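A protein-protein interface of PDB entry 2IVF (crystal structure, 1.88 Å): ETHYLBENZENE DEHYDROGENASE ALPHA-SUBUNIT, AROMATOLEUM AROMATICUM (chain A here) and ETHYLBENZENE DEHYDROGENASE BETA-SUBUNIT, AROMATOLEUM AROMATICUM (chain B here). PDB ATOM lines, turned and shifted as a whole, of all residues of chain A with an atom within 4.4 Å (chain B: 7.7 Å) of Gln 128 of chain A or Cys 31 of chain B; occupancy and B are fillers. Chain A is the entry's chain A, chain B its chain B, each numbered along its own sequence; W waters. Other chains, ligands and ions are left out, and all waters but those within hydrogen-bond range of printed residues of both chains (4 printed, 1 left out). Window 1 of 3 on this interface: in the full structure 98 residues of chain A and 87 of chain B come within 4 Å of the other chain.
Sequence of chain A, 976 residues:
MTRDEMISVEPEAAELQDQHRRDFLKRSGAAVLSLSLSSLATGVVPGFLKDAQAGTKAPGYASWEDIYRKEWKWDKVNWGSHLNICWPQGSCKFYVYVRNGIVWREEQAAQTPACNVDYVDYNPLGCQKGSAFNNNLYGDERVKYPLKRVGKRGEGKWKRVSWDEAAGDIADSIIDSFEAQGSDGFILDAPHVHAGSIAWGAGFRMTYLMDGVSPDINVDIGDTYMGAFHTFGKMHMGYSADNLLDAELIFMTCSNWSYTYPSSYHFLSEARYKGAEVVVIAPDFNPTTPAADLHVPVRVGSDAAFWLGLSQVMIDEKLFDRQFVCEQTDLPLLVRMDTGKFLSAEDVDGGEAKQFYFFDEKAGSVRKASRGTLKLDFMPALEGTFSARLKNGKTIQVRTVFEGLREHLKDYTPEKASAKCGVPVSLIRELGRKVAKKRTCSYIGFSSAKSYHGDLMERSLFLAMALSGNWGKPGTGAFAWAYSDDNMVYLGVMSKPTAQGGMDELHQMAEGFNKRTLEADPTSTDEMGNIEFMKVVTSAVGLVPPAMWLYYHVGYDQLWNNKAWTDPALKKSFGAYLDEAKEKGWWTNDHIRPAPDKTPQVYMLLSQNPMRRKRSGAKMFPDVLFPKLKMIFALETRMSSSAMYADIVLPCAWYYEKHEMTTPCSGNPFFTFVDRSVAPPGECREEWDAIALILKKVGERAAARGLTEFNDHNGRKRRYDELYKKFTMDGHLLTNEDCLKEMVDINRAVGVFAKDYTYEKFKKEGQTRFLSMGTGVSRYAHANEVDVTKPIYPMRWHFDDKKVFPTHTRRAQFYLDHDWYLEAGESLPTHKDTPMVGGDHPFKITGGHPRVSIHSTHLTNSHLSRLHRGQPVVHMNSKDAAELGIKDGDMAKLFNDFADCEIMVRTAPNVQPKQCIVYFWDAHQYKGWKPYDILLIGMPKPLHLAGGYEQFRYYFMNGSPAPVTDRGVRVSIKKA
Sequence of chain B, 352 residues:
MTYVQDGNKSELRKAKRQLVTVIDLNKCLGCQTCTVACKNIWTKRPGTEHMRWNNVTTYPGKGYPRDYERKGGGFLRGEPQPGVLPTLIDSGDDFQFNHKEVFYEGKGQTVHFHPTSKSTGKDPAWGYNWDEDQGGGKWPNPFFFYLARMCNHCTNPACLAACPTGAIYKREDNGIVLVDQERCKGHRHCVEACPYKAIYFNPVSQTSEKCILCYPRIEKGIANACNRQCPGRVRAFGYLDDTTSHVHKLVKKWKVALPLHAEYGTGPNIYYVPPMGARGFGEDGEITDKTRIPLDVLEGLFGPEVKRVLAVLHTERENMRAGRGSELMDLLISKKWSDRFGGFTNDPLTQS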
ATOM      1  N   CYS A 127       1.701   8.402 -12.943  1.00  0.00           N
ATOM      2  CA  CYS A 127       2.127   7.801 -11.705  1.00  0.00           C
ATOM      3  C   CYS A 127       0.986   7.835 -10.712  1.00  0.00           C
ATOM      4  O   CYS A 127      -0.116   8.375 -11.010  1.00  0.00           O
ATOM      5  CB  CYS A 127       3.314   8.498 -11.157  1.00  0.00           C
ATOM      6  SG  CYS A 127       2.991  10.055 -10.249  1.00  0.00           S
ATOM      7  N   GLN A 128       1.233   7.272  -9.541  1.00  0.00           N
ATOM      8  CA  GLN A 128       0.122   7.080  -8.602  1.00  0.00           C
ATOM      9  C   GLN A 128      -0.288   8.416  -7.935  1.00  0.00           C
ATOM     10  O   GLN A 128      -1.449   8.603  -7.563  1.00  0.00           O
ATOM     11  CB  GLN A 128       0.445   5.971  -7.568  1.00  0.00           C
ATOM     12  CG  GLN A 128       1.427   6.396  -6.432  1.00  0.00           C
ATOM     13  CD  GLN A 128       2.873   6.472  -6.869  1.00  0.00           C
ATOM     14  OE1 GLN A 128       3.172   6.830  -8.020  1.00  0.00           O
ATOM     15  NE2 GLN A 128       3.788   6.208  -5.948  1.00  0.00           N
ATOM     16  N   LYS A 129       0.653   9.354  -7.814  1.00  0.00           N
ATOM     17  CA  LYS A 129       0.346  10.615  -7.209  1.00  0.00           C
ATOM     18  C   LYS A 129      -0.532  11.390  -8.186  1.00  0.00           C
ATOM     19  O   LYS A 129      -1.572  11.898  -7.801  1.00  0.00           O
ATOM     20  CB  LYS A 129       1.597  11.396  -6.916  1.00  0.00           C
ATOM     21  CG  LYS A 129       2.357  10.918  -5.692  1.00  0.00           C
ATOM     22  CD  LYS A 129       3.273   9.721  -5.997  1.00  0.00           C
ATOM     23  CE  LYS A 129       4.427  10.079  -6.940  1.00  0.00           C
ATOM     24  NZ  LYS A 129       5.240   8.873  -7.286  1.00  0.00           N
ATOM     25  N   GLY A 130      -0.096  11.456  -9.437  1.00  0.00           N
ATOM     26  CA  GLY A 130      -0.849  12.137 -10.512  1.00  0.00           C
ATOM     27  C   GLY A 130      -2.226  11.557 -10.735  1.00  0.00           C
ATOM     28  O   GLY A 130      -3.216  12.288 -10.939  1.00  0.00           O
ATOM     29  N   SER A 131      -2.288  10.230 -10.700  1.00  0.00           N
ATOM     30  CA  SER A 131      -3.521   9.489 -10.975  1.00  0.00           C
ATOM     31  C   SER A 131      -4.525   9.526  -9.809  1.00  0.00           C
ATOM     32  O   SER A 131      -5.641   8.985  -9.938  1.00  0.00           O
ATOM     33  CB  SER A 131      -3.172   8.048 -11.333  1.00  0.00           C
ATOM     34  OG  SER A 131      -2.463   7.988 -12.562  1.00  0.00           O
ATOM     35  N   ALA A 132      -4.132  10.139  -8.696  1.00  0.00           N
ATOM     36  CA  ALA A 132      -5.010  10.349  -7.519  1.00  0.00           C
ATOM     37  C   ALA A 132      -5.052  11.808  -7.081  1.00  0.00           C
ATOM     38  O   ALA A 132      -5.536  12.130  -5.994  1.00  0.00           O
ATOM     39  CB  ALA A 132      -4.504   9.513  -6.359  1.00  0.00           C
ATOM     40  N   PRO A 262       8.677   6.919 -12.519  1.00  0.00           N
ATOM     41  CA  PRO A 262       7.731   5.852 -12.853  1.00  0.00           C
ATOM     42  C   PRO A 262       7.080   6.004 -14.202  1.00  0.00           C
ATOM     43  O   PRO A 262       6.717   5.014 -14.786  1.00  0.00           O
ATOM     44  CB  PRO A 262       6.696   5.914 -11.735  1.00  0.00           C
ATOM     45  CG  PRO A 262       6.787   7.325 -11.175  1.00  0.00           C
ATOM     46  CD  PRO A 262       8.232   7.723 -11.367  1.00  0.00           C
ATOM     47  N   ARG A 851       8.894   7.778  -3.109  1.00  0.00           N
ATOM     48  CA  ARG A 851       7.938   7.115  -3.977  1.00  0.00           C
ATOM     49  C   ARG A 851       6.564   7.738  -3.788  1.00  0.00           C
ATOM     50  O   ARG A 851       5.824   7.947  -4.769  1.00  0.00           O
ATOM     51  CB  ARG A 851       7.805   5.665  -3.611  1.00  0.00           C
ATOM     52  CG  ARG A 851       6.641   5.032  -4.309  1.00  0.00           C
ATOM     53  CD  ARG A 851       6.548   3.556  -4.004  1.00  0.00           C
ATOM     54  NE  ARG A 851       7.462   2.783  -4.780  1.00  0.00           N
ATOM     55  CZ  ARG A 851       8.000   1.640  -4.408  1.00  0.00           C
ATOM     56  NH1 ARG A 851       7.887   1.181  -3.164  1.00  0.00           N
ATOM     57  NH2 ARG A 851       8.799   1.035  -5.256  1.00  0.00           N
ATOM     58  N   LEU A 864      -3.332   9.343  -0.522  1.00  0.00           N
ATOM     59  CA  LEU A 864      -2.061   8.843  -1.020  1.00  0.00           C
ATOM     60  C   LEU A 864      -1.242   8.311   0.114  1.00  0.00           C
ATOM     61  O   LEU A 864      -0.413   7.408  -0.073  1.00  0.00           O
ATOM     62  CB  LEU A 864      -1.313   9.941  -1.815  1.00  0.00           C
ATOM     63  CG  LEU A 864      -1.900  10.167  -3.223  1.00  0.00           C
ATOM     64  CD1 LEU A 864      -1.425  11.458  -3.930  1.00  0.00           C
ATOM     65  CD2 LEU A 864      -1.552   8.884  -4.079  1.00  0.00           C
ATOM     66  N   LEU A 867      -1.208   4.559   0.928  1.00  0.00           N
ATOM     67  CA  LEU A 867      -0.385   3.632   0.111  1.00  0.00           C
ATOM     68  C   LEU A 867       0.870   3.213   0.893  1.00  0.00           C
ATOM     69  O   LEU A 867       1.644   2.415   0.418  1.00  0.00           O
ATOM     70  CB  LEU A 867       0.025   4.332  -1.192  1.00  0.00           C
ATOM     71  CG  LEU A 867      -1.216   4.541  -2.093  1.00  0.00           C
ATOM     72  CD1 LEU A 867      -0.835   5.152  -3.446  1.00  0.00           C
ATOM     73  CD2 LEU A 867      -2.017   3.275  -2.359  1.00  0.00           C
ATOM     74  N   CYS B  28       7.224  -4.659 -13.133  1.00  0.00           N
ATOM     75  CA  CYS B  28       6.499  -3.964 -12.116  1.00  0.00           C
ATOM     76  C   CYS B  28       7.440  -3.211 -11.221  1.00  0.00           C
ATOM     77  O   CYS B  28       8.416  -3.751 -10.760  1.00  0.00           O
ATOM     78  CB  CYS B  28       5.588  -4.881 -11.271  1.00  0.00           C
ATOM     79  SG  CYS B  28       4.690  -3.948 -10.045  1.00  0.00           S
ATOM     80  N   LEU B  29       7.147  -1.933 -11.049  1.00  0.00           N
ATOM     81  CA  LEU B  29       7.967  -1.055 -10.235  1.00  0.00           C
ATOM     82  C   LEU B  29       7.315  -0.630  -8.914  1.00  0.00           C
ATOM     83  O   LEU B  29       7.815   0.254  -8.211  1.00  0.00           O
ATOM     84  CB  LEU B  29       8.399   0.155 -11.043  1.00  0.00           C
ATOM     85  CG  LEU B  29       7.263   0.969 -11.643  1.00  0.00           C
ATOM     86  CD1 LEU B  29       7.608   2.370 -11.562  1.00  0.00           C
ATOM     87  CD2 LEU B  29       7.020   0.552 -13.128  1.00  0.00           C
ATOM     88  N   GLY B  30       6.234  -1.303  -8.540  1.00  0.00           N
ATOM     89  CA  GLY B  30       5.623  -1.073  -7.244  1.00  0.00           C
ATOM     90  C   GLY B  30       5.088   0.347  -7.041  1.00  0.00           C
ATOM     91  O   GLY B  30       4.984   0.793  -5.912  1.00  0.00           O
ATOM     92  N   CYS B  31       4.699   1.008  -8.124  1.00  0.00           N
ATOM     93  CA  CYS B  31       4.278   2.429  -8.067  1.00  0.00           C
ATOM     94  C   CYS B  31       2.857   2.594  -7.556  1.00  0.00           C
ATOM     95  O   CYS B  31       2.462   3.702  -7.300  1.00  0.00           O
ATOM     96  CB  CYS B  31       4.412   3.099  -9.449  1.00  0.00           C
ATOM     97  SG  CYS B  31       3.211   2.438 -10.686  1.00  0.00           S
ATOM     98  N   GLN B  32       2.052   1.521  -7.470  1.00  0.00           N
ATOM     99  CA  GLN B  32       0.662   1.609  -6.957  1.00  0.00           C
ATOM    100  C   GLN B  32      -0.303   2.438  -7.858  1.00  0.00           C
ATOM    101  O   GLN B  32      -1.401   2.764  -7.438  1.00  0.00           O
ATOM    102  CB  GLN B  32       0.630   2.238  -5.535  1.00  0.00           C
ATOM    103  CG  GLN B  32       1.521   1.590  -4.438  1.00  0.00           C
ATOM    104  CD  GLN B  32       0.959   0.251  -3.960  1.00  0.00           C
ATOM    105  OE1 GLN B  32      -0.242   0.046  -4.045  1.00  0.00           O
ATOM    106  NE2 GLN B  32       1.813  -0.663  -3.480  1.00  0.00           N
ATOM    107  N   THR B  33       0.086   2.794  -9.083  1.00  0.00           N
ATOM    108  CA  THR B  33      -0.832   3.506  -9.960  1.00  0.00           C
ATOM    109  C   THR B  33      -2.081   2.680 -10.212  1.00  0.00           C
ATOM    110  O   THR B  33      -3.197   3.213 -10.202  1.00  0.00           O
ATOM    111  CB  THR B  33      -0.186   3.951 -11.276  1.00  0.00           C
ATOM    112  OG1 THR B  33       1.018   4.625 -10.985  1.00  0.00           O
ATOM    113  CG2 THR B  33      -1.105   4.894 -12.048  1.00  0.00           C
ATOM    114  N   CYS B  34      -1.898   1.377 -10.418  1.00  0.00           N
ATOM    115  CA  CYS B  34      -3.010   0.482 -10.573  1.00  0.00           C
ATOM    116  C   CYS B  34      -3.971   0.492  -9.351  1.00  0.00           C
ATOM    117  O   CYS B  34      -5.203   0.474  -9.528  1.00  0.00           O
ATOM    118  CB  CYS B  34      -2.518  -0.931 -10.904  1.00  0.00           C
ATOM    119  SG  CYS B  34      -1.294  -1.504  -9.673  1.00  0.00           S
ATOM    120  N   THR B  35      -3.404   0.613  -8.151  1.00  0.00           N
ATOM    121  CA  THR B  35      -4.158   0.700  -6.901  1.00  0.00           C
ATOM    122  C   THR B  35      -5.069   1.911  -6.908  1.00  0.00           C
ATOM    123  O   THR B  35      -6.321   1.799  -6.671  1.00  0.00           O
ATOM    124  CB  THR B  35      -3.185   0.720  -5.729  1.00  0.00           C
ATOM    125  OG1 THR B  35      -2.332  -0.426  -5.865  1.00  0.00           O
ATOM    126  CG2 THR B  35      -3.946   0.730  -4.356  1.00  0.00           C
ATOM    127  N   VAL B  36      -4.480   3.039  -7.221  1.00  0.00           N
ATOM    128  CA  VAL B  36      -5.244   4.302  -7.248  1.00  0.00           C
ATOM    129  C   VAL B  36      -6.198   4.380  -8.435  1.00  0.00           C
ATOM    130  O   VAL B  36      -7.243   5.023  -8.325  1.00  0.00           O
ATOM    131  CB  VAL B  36      -4.360   5.575  -7.148  1.00  0.00           C
ATOM    132  CG1 VAL B  36      -3.360   5.497  -5.935  1.00  0.00           C
ATOM    133  CG2 VAL B  36      -3.663   5.914  -8.468  1.00  0.00           C
ATOM    134  N   ALA B  37      -5.847   3.735  -9.558  1.00  0.00           N
ATOM    135  CA  ALA B  37      -6.695   3.715 -10.753  1.00  0.00           C
ATOM    136  C   ALA B  37      -8.019   3.078 -10.369  1.00  0.00           C
ATOM    137  O   ALA B  37      -9.079   3.627 -10.595  1.00  0.00           O
ATOM    138  CB  ALA B  37      -5.998   2.900 -11.925  1.00  0.00           C
ATOM    139  N   ASN B  40     -10.009   5.132  -7.340  1.00  0.00           N
ATOM    140  CA  ASN B  40     -10.579   6.412  -7.711  1.00  0.00           C
ATOM    141  C   ASN B  40     -11.753   6.325  -8.649  1.00  0.00           C
ATOM    142  O   ASN B  40     -12.395   7.340  -8.908  1.00  0.00           O
ATOM    143  CB  ASN B  40      -9.472   7.359  -8.207  1.00  0.00           C
ATOM    144  CG  ASN B  40      -8.674   7.921  -7.041  1.00  0.00           C
ATOM    145  OD1 ASN B  40      -9.097   8.907  -6.417  1.00  0.00           O
ATOM    146  ND2 ASN B  40      -7.593   7.235  -6.669  1.00  0.00           N
ATOM    147  N   VAL B  56      -1.239  -3.952  -4.449  1.00  0.00           N
ATOM    148  CA  VAL B  56       0.172  -4.200  -4.782  1.00  0.00           C
ATOM    149  C   VAL B  56       1.005  -4.212  -3.542  1.00  0.00           C
ATOM    150  O   VAL B  56       0.974  -3.270  -2.768  1.00  0.00           O
ATOM    151  CB  VAL B  56       0.764  -3.167  -5.755  1.00  0.00           C
ATOM    152  CG1 VAL B  56       2.123  -3.626  -6.168  1.00  0.00           C
ATOM    153  CG2 VAL B  56      -0.116  -2.928  -6.979  1.00  0.00           C
ATOM    154  N   ASN B 129       0.030  -2.188   2.606  1.00  0.00           N
ATOM    155  CA  ASN B 129       1.376  -2.011   2.089  1.00  0.00           C
ATOM    156  C   ASN B 129       2.366  -1.595   3.176  1.00  0.00           C
ATOM    157  O   ASN B 129       3.354  -0.915   2.926  1.00  0.00           O
ATOM    158  CB  ASN B 129       1.366  -0.983   0.942  1.00  0.00           C
ATOM    159  CG  ASN B 129       2.594  -1.076   0.085  1.00  0.00           C
ATOM    160  OD1 ASN B 129       3.186  -2.152  -0.008  1.00  0.00           O
ATOM    161  ND2 ASN B 129       3.022   0.041  -0.516  1.00  0.00           N
ATOM    162  N   GLU B 132       6.037  -2.659   2.770  1.00  0.00           N
ATOM    163  CA  GLU B 132       6.626  -2.141   1.573  1.00  0.00           C
ATOM    164  C   GLU B 132       8.152  -2.169   1.611  1.00  0.00           C
ATOM    165  O   GLU B 132       8.763  -1.721   2.581  1.00  0.00           O
ATOM    166  CB  GLU B 132       6.123  -0.723   1.329  1.00  0.00           C
ATOM    167  CG  GLU B 132       6.469  -0.147  -0.044  1.00  0.00           C
ATOM    168  CD  GLU B 132       5.866   1.208  -0.255  1.00  0.00           C
ATOM    169  OE1 GLU B 132       5.709   1.948   0.743  1.00  0.00           O
ATOM    170  OE2 GLU B 132       5.590   1.545  -1.414  1.00  0.00           O
ATOM    171  N   TYR B 146       7.598  -6.718  -6.739  1.00  0.00           N
ATOM    172  CA  TYR B 146       6.295  -6.199  -6.405  1.00  0.00           C
ATOM    173  C   TYR B 146       5.225  -7.064  -7.009  1.00  0.00           C
ATOM    174  O   TYR B 146       5.368  -7.554  -8.152  1.00  0.00           O
ATOM    175  CB  TYR B 146       6.186  -4.756  -6.849  1.00  0.00           C
ATOM    176  CG  TYR B 146       7.244  -3.884  -6.220  1.00  0.00           C
ATOM    177  CD1 TYR B 146       7.171  -3.568  -4.869  1.00  0.00           C
ATOM    178  CD2 TYR B 146       8.290  -3.353  -6.971  1.00  0.00           C
ATOM    179  CE1 TYR B 146       8.143  -2.786  -4.265  1.00  0.00           C
ATOM    180  CE2 TYR B 146       9.276  -2.504  -6.373  1.00  0.00           C
ATOM    181  CZ  TYR B 146       9.169  -2.231  -5.022  1.00  0.00           C
ATOM    182  OH  TYR B 146      10.110  -1.422  -4.431  1.00  0.00           O
ATOM    183  N   GLN B 229      -4.024   1.877 -16.848  1.00  0.00           N
ATOM    184  CA  GLN B 229      -3.250   2.942 -16.192  1.00  0.00           C
ATOM    185  C   GLN B 229      -1.857   2.609 -15.655  1.00  0.00           C
ATOM    186  O   GLN B 229      -1.197   3.450 -15.036  1.00  0.00           O
ATOM    187  CB  GLN B 229      -4.086   3.578 -15.087  1.00  0.00           C
ATOM    188  CG  GLN B 229      -5.356   4.267 -15.646  1.00  0.00           C
ATOM    189  CD  GLN B 229      -6.092   5.115 -14.647  1.00  0.00           C
ATOM    190  OE1 GLN B 229      -7.240   4.844 -14.347  1.00  0.00           O
ATOM    191  NE2 GLN B 229      -5.408   6.129 -14.076  1.00  0.00           N
ATOM    192  N   CYS B 230      -1.375   1.408 -15.922  1.00  0.00           N
ATOM    193  CA  CYS B 230      -0.129   0.944 -15.417  1.00  0.00           C
ATOM    194  C   CYS B 230       0.980   1.599 -16.250  1.00  0.00           C
ATOM    195  O   CYS B 230       1.123   1.288 -17.454  1.00  0.00           O
ATOM    196  CB  CYS B 230      -0.040  -0.526 -15.591  1.00  0.00           C
ATOM    197  SG  CYS B 230       1.590  -1.222 -15.311  1.00  0.00           S
ATOM    198  N   PRO B 231       1.720   2.492 -15.626  1.00  0.00           N
ATOM    199  CA  PRO B 231       2.808   3.119 -16.338  1.00  0.00           C
ATOM    200  C   PRO B 231       3.970   2.222 -16.662  1.00  0.00           C
ATOM    201  O   PRO B 231       4.767   2.567 -17.529  1.00  0.00           O
ATOM    202  CB  PRO B 231       3.268   4.219 -15.416  1.00  0.00           C
ATOM    203  CG  PRO B 231       2.361   4.241 -14.270  1.00  0.00           C
ATOM    204  CD  PRO B 231       1.595   3.004 -14.256  1.00  0.00           C
ATOM    205  N   GLY B 232       4.125   1.133 -15.927  1.00  0.00           N
ATOM    206  CA  GLY B 232       5.205   0.208 -16.167  1.00  0.00           C
ATOM    207  C   GLY B 232       4.996  -0.662 -17.399  1.00  0.00           C
ATOM    208  O   GLY B 232       5.921  -1.348 -17.815  1.00  0.00           O
ATOM    209  N   VAL B 234       3.184  -3.238 -17.734  1.00  0.00           N
ATOM    210  CA  VAL B 234       3.316  -4.564 -17.138  1.00  0.00           C
ATOM    211  C   VAL B 234       2.165  -5.474 -17.506  1.00  0.00           C
ATOM    212  O   VAL B 234       2.268  -6.694 -17.419  1.00  0.00           O
ATOM    213  CB  VAL B 234       3.300  -4.290 -15.614  1.00  0.00           C
ATOM    214  CG1 VAL B 234       2.900  -5.435 -14.774  1.00  0.00           C
ATOM    215  CG2 VAL B 234       4.580  -3.573 -15.247  1.00  0.00           C
HETATM  216  O   HOH W   1       7.255   3.278 -16.761  1.00  0.00           O
HETATM  217  O   HOH W   2       7.378   2.877  -7.637  1.00  0.00           O
HETATM  218  O   HOH W   3       3.540   3.176  -1.682  1.00  0.00           O
HETATM  219  O   HOH W   4      -6.920   7.492 -11.751  1.00  0.00           O
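The backbone carbonyl oxygen of Cys 31 of chain B sits close to the side-chain amide nitrogen of Gln 128 of chain A, at 3.1 Å.
The backbone NH of Gln 128 of chain A is in hydrogen-bond range of the side-chain hydroxyl of Thr 33 of chain B, 3.0 Å away.
NH2 of Arg 851 of chain A is in hydrogen-bond range of O of Leu 29 of chain B, at 3.2 Å.
NE of Arg 851 of chain A is in hydrogen-bond range of O of Gly 30 of chain B, 3.4 Å away.
The guanidinium group of Arg 851 of chain A lies within salt-bridge range of the side-chain carboxylate of Glu 132 of chain B (2.9 Å).
The guanidinium group of Arg 851 of chain A sits at hydrogen-bond distance from the side-chain hydroxyl of Tyr 146 of chain B, at 2.9 Å.
O of Leu 867 of chain A sits at hydrogen-bond distance from ND2 of Asn 129 of chain B (2.9 Å).
O of Cys 127 of chain A lies within hydrogen-bond range of OG of Ser 131 of chain A (2.8 Å).
The backbone carbonyl oxygen of Arg 851 of chain A is in hydrogen-bond range of the side-chain amide nitrogen of Gln 128 of chain A (2.9 Å).
OG1 of Thr 33 of chain B lies close to SG of Cys 31 of chain B.
The side-chain amide nitrogen of Gln 32 of chain B is in hydrogen-bond range of the backbone carbonyl oxygen of Val 56 of chain B (2.8 Å).
The side-chain amide nitrogen (NE2) of Gln 32 of chain B sits close to the side-chain amide nitrogen (ND2) of Asn 129 of chain B, at 3.3 Å.
The side-chain carboxylate of Glu 132 of chain B sits close to the side-chain amide nitrogen of Asn 129 of chain B, at 3.1 Å.
Among the printed residues, pairs that only touch across the chains: Cys 127 of chain A with Thr 33 of chain B (3.2 Å), Ser 131 of chain A with Thr 33 of chain B (3.4 Å), Leu 867 of chain A with Val 36 of chain B (3.6 Å), Pro 262 of chain A with Pro 231 of chain B (3.6 Å), Gln 128 of chain A with Val 36 of chain B (3.6 Å), Ser 131 of chain A with Val 36 of chain B (3.6 Å), Gln 128 of chain A with Gln 32 of chain B (3.6 Å), Pro 262 of chain A with Leu 29 of chain B (3.7 Å), Leu 867 of chain A with Thr 35 of chain B (3.8 Å), Ser 131 of chain A with Gln 229 of chain B (3.8 Å), Ala 132 of chain A with Asn 40 of chain B (3.9 Å) and Leu 867 of chain A with Gln 32 of chain B (3.9 Å).
Of chain B, only Thr 33 comes within 4 Å of Cys 127 of chain A.
Of the printed residues of chain B, Gln 128 of chain A touches Cys 31 (2.8 Å), Gln 32 (3.6 Å), Thr 33 (3.0 Å) and Val 36 (3.6 Å).
Printed residues of chain A within 4 Å of Gly 30 of chain B: Arg 851.
Of chain A, only Gln 128 (2.8 Å) comes within 4 Å of Cys 31 of chain B.
Printed residues of chain A within 4 Å of Val 36 of chain B: Gln 128 (3.6 Å), Ser 131 (3.6 Å) and Leu 867 (3.6 Å).
The nearest residue of chain B that does not touch Gln 128 of chain A is Gly 30 of chain B (5.5 Å).
Of the 10 printed residues of chain A, 7 touch a printed residue of chain B.
Hydrophobic or aromatic side chains of chain A within 4 Å of the printed part of chain B: Ala 132, Pro 262 and Leu 867.
Along chain A the printed residues that touch a printed residue of chain B span positions 127 to 867.
Of the 20 printed residues of chain B, 13 touch a printed residue of chain A.
Water W3 lies within hydrogen-bond range of OE2 of Glu 132 of chain B (2.6 Å), O of Leu 867 of chain A (2.9 Å) and ND2 of Asn 129 of chain B (3.4 Å).
Water W4 bridges O of Ser 131 of chain A and NE2 of Gln 229 of chain B.
Water W1 lies within hydrogen-bond range of O of Pro 262 of chain A (2.7 Å) and O of Pro 231 of chain B (2.7 Å).
Water W2 lies within hydrogen-bond range of O of Leu 29 of chain B, NE of Arg 851 of chain A and N of Cys 31 of chain B.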
